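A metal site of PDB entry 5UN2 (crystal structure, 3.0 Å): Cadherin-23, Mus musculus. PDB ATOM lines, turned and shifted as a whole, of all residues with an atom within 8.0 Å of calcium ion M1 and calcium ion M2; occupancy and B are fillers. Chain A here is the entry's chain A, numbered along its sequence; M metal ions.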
ATOM      1  N   GLU A 232      18.852 -18.036  17.976  1.00  0.00           N
ATOM      2  CA  GLU A 232      19.720 -17.018  17.382  1.00  0.00           C
ATOM      3  C   GLU A 232      19.287 -15.584  17.811  1.00  0.00           C
ATOM      4  O   GLU A 232      20.123 -14.669  17.898  1.00  0.00           O
ATOM      5  CB  GLU A 232      19.866 -17.188  15.851  1.00  0.00           C
ATOM      6  CG  GLU A 232      18.576 -17.127  15.046  1.00  0.00           C
ATOM      7  CD  GLU A 232      18.811 -17.012  13.535  1.00  0.00           C
ATOM      8  OE1 GLU A 232      17.991 -17.562  12.740  1.00  0.00           O
ATOM      9  OE2 GLU A 232      19.804 -16.351  13.147  1.00  0.00           O
ATOM     10  N   SER A 233      18.016 -15.420  18.165  1.00  0.00           N
ATOM     11  CA  SER A 233      17.490 -14.153  18.699  1.00  0.00           C
ATOM     12  C   SER A 233      17.889 -13.807  20.141  1.00  0.00           C
ATOM     13  O   SER A 233      17.511 -12.742  20.625  1.00  0.00           O
ATOM     14  CB  SER A 233      15.961 -14.130  18.586  1.00  0.00           C
ATOM     15  OG  SER A 233      15.364 -14.914  19.615  1.00  0.00           O
ATOM     16  N   LEU A 293      24.207 -13.366  18.178  1.00  0.00           N
ATOM     17  CA  LEU A 293      24.230 -14.684  17.511  1.00  0.00           C
ATOM     18  C   LEU A 293      23.456 -14.667  16.186  1.00  0.00           C
ATOM     19  O   LEU A 293      22.400 -14.059  16.098  1.00  0.00           O
ATOM     20  CB  LEU A 293      23.592 -15.733  18.420  1.00  0.00           C
ATOM     21  CG  LEU A 293      24.175 -15.882  19.812  1.00  0.00           C
ATOM     22  CD1 LEU A 293      23.290 -16.754  20.681  1.00  0.00           C
ATOM     23  CD2 LEU A 293      25.573 -16.478  19.735  1.00  0.00           C
ATOM     24  N   ASN A 294      24.007 -15.334  15.177  1.00  0.00           N
ATOM     25  CA  ASN A 294      23.368 -15.519  13.866  1.00  0.00           C
ATOM     26  C   ASN A 294      23.563 -16.968  13.448  1.00  0.00           C
ATOM     27  O   ASN A 294      24.709 -17.401  13.241  1.00  0.00           O
ATOM     28  CB  ASN A 294      23.971 -14.587  12.818  1.00  0.00           C
ATOM     29  CG  ASN A 294      23.269 -14.672  11.471  1.00  0.00           C
ATOM     30  OD1 ASN A 294      22.193 -15.246  11.338  1.00  0.00           O
ATOM     31  ND2 ASN A 294      23.865 -14.078  10.460  1.00  0.00           N
ATOM     32  N   ARG A 295      22.466 -17.716  13.317  1.00  0.00           N
ATOM     33  CA  ARG A 295      22.519 -19.118  12.898  1.00  0.00           C
ATOM     34  C   ARG A 295      23.108 -19.274  11.500  1.00  0.00           C
ATOM     35  O   ARG A 295      23.802 -20.247  11.200  1.00  0.00           O
ATOM     36  CB  ARG A 295      21.122 -19.749  12.920  1.00  0.00           C
ATOM     37  CG  ARG A 295      21.167 -21.165  12.395  1.00  0.00           C
ATOM     38  CD  ARG A 295      19.993 -22.045  12.739  1.00  0.00           C
ATOM     39  NE  ARG A 295      20.483 -23.428  12.795  1.00  0.00           N
ATOM     40  CZ  ARG A 295      20.835 -24.164  11.737  1.00  0.00           C
ATOM     41  NH1 ARG A 295      21.298 -25.407  11.938  1.00  0.00           N
ATOM     42  NH2 ARG A 295      20.738 -23.693  10.487  1.00  0.00           N
ATOM     43  N   GLU A 296      22.816 -18.300  10.656  1.00  0.00           N
ATOM     44  CA  GLU A 296      23.228 -18.313   9.269  1.00  0.00           C
ATOM     45  C   GLU A 296      24.738 -18.090   9.116  1.00  0.00           C
ATOM     46  O   GLU A 296      25.311 -18.365   8.052  1.00  0.00           O
ATOM     47  CB  GLU A 296      22.424 -17.271   8.491  1.00  0.00           C
ATOM     48  CG  GLU A 296      20.984 -17.692   8.244  1.00  0.00           C
ATOM     49  CD  GLU A 296      20.131 -17.747   9.499  1.00  0.00           C
ATOM     50  OE1 GLU A 296      19.598 -18.842   9.803  1.00  0.00           O
ATOM     51  OE2 GLU A 296      19.952 -16.710  10.175  1.00  0.00           O
ATOM     52  N   LEU A 297      25.366 -17.585  10.183  1.00  0.00           N
ATOM     53  CA  LEU A 297      26.805 -17.528  10.315  1.00  0.00           C
ATOM     54  C   LEU A 297      27.361 -18.733  11.047  1.00  0.00           C
ATOM     55  O   LEU A 297      28.215 -19.451  10.524  1.00  0.00           O
ATOM     56  CB  LEU A 297      27.214 -16.246  11.035  1.00  0.00           C
ATOM     57  CG  LEU A 297      28.705 -15.915  11.124  1.00  0.00           C
ATOM     58  CD1 LEU A 297      29.302 -15.794   9.742  1.00  0.00           C
ATOM     59  CD2 LEU A 297      28.859 -14.626  11.922  1.00  0.00           C
ATOM     60  N   ILE A 330      22.722 -23.864  17.805  1.00  0.00           N
ATOM     61  CA  ILE A 330      21.971 -22.640  17.592  1.00  0.00           C
ATOM     62  C   ILE A 330      20.699 -22.903  16.777  1.00  0.00           C
ATOM     63  O   ILE A 330      20.779 -23.392  15.630  1.00  0.00           O
ATOM     64  CB  ILE A 330      22.807 -21.543  16.894  1.00  0.00           C
ATOM     65  CG1 ILE A 330      24.052 -21.194  17.717  1.00  0.00           C
ATOM     66  CG2 ILE A 330      21.977 -20.289  16.650  1.00  0.00           C
ATOM     67  CD1 ILE A 330      23.785 -20.360  18.949  1.00  0.00           C
ATOM     68  N   LEU A 331      19.552 -22.519  17.375  1.00  0.00           N
ATOM     69  CA  LEU A 331      18.216 -22.665  16.779  1.00  0.00           C
ATOM     70  C   LEU A 331      17.810 -21.535  15.792  1.00  0.00           C
ATOM     71  O   LEU A 331      18.160 -20.365  16.003  1.00  0.00           O
ATOM     72  CB  LEU A 331      17.172 -22.800  17.891  1.00  0.00           C
ATOM     73  CG  LEU A 331      17.366 -23.962  18.863  1.00  0.00           C
ATOM     74  CD1 LEU A 331      16.401 -23.831  20.032  1.00  0.00           C
ATOM     75  CD2 LEU A 331      17.184 -25.277  18.142  1.00  0.00           C
ATOM     76  N   ASP A 332      17.072 -21.900  14.735  1.00  0.00           N
ATOM     77  CA  ASP A 332      16.789 -20.977  13.615  1.00  0.00           C
ATOM     78  C   ASP A 332      15.607 -20.105  13.930  1.00  0.00           C
ATOM     79  O   ASP A 332      14.679 -20.539  14.573  1.00  0.00           O
ATOM     80  CB  ASP A 332      16.501 -21.728  12.313  1.00  0.00           C
ATOM     81  CG  ASP A 332      16.451 -20.797  11.097  1.00  0.00           C
ATOM     82  OD1 ASP A 332      17.067 -19.708  11.131  1.00  0.00           O
ATOM     83  OD2 ASP A 332      15.784 -21.158  10.094  1.00  0.00           O
ATOM     84  N   VAL A 333      15.641 -18.867  13.469  1.00  0.00           N
ATOM     85  CA  VAL A 333      14.466 -18.000  13.531  1.00  0.00           C
ATOM     86  C   VAL A 333      14.117 -17.600  12.100  1.00  0.00           C
ATOM     87  O   VAL A 333      15.019 -17.249  11.324  1.00  0.00           O
ATOM     88  CB  VAL A 333      14.704 -16.795  14.467  1.00  0.00           C
ATOM     89  CG1 VAL A 333      13.520 -15.834  14.438  1.00  0.00           C
ATOM     90  CG2 VAL A 333      14.961 -17.264  15.891  1.00  0.00           C
ATOM     91  N   ASN A 334      12.830 -17.702  11.740  1.00  0.00           N
ATOM     92  CA  ASN A 334      12.352 -17.382  10.389  1.00  0.00           C
ATOM     93  C   ASN A 334      10.811 -17.102  10.380  1.00  0.00           C
ATOM     94  O   ASN A 334      10.178 -17.084  11.435  1.00  0.00           O
ATOM     95  CB  ASN A 334      12.809 -18.445   9.382  1.00  0.00           C
ATOM     96  CG  ASN A 334      12.286 -19.824   9.706  1.00  0.00           C
ATOM     97  OD1 ASN A 334      11.132 -20.150   9.399  1.00  0.00           O
ATOM     98  ND2 ASN A 334      13.128 -20.655  10.301  1.00  0.00           N
ATOM     99  N   ASP A 335      10.250 -16.893   9.190  1.00  0.00           N
ATOM    100  CA  ASP A 335       8.928 -16.245   9.007  1.00  0.00           C
ATOM    101  C   ASP A 335       7.742 -17.081   9.513  1.00  0.00           C
ATOM    102  O   ASP A 335       7.069 -17.762   8.741  1.00  0.00           O
ATOM    103  CB  ASP A 335       8.722 -15.855   7.521  1.00  0.00           C
ATOM    104  CG  ASP A 335       9.923 -15.102   6.926  1.00  0.00           C
ATOM    105  OD1 ASP A 335      10.878 -14.748   7.681  1.00  0.00           O
ATOM    106  OD2 ASP A 335       9.933 -14.868   5.699  1.00  0.00           O
HETATM  107 CA    CA M   1      20.168 -14.514  11.666  1.00  0.00          CA
HETATM  108 CA    CA M   2      17.277 -17.456  10.414  1.00  0.00          CA
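OD1 of Asn 294 binds calcium ion M1 (2.2 Å).
OE2 of Glu 232 is bound to calcium ion M1, 2.4 Å away.
The side-chain carboxylate (OE2) of Glu 296 is bound to calcium ion M1, 2.7 Å away.
Calcium ion M2 is bound by OD1 of Asp 332, OE1 of Glu 232, O of Val 333, OE1 of Glu 296 and OE2 of Glu 296.
Within 4 Å of calcium ion M2: Glu 232, Glu 296, Asp 332 and Val 333.
Along chain A the residues within 4 Å of calcium ion M2 span positions 232 to 333.
The backbone NH (N) of Glu 232 is in hydrogen-bond range of the backbone carbonyl oxygen (O) of Leu 331 (3.1 Å).
The side-chain amide nitrogen of Asn 334 lies within hydrogen-bond range of the side-chain carboxylate of Asp 332, 2.7 Å away.
OE2 of Glu 232 lies close to N of Arg 295 (3.0 Å).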
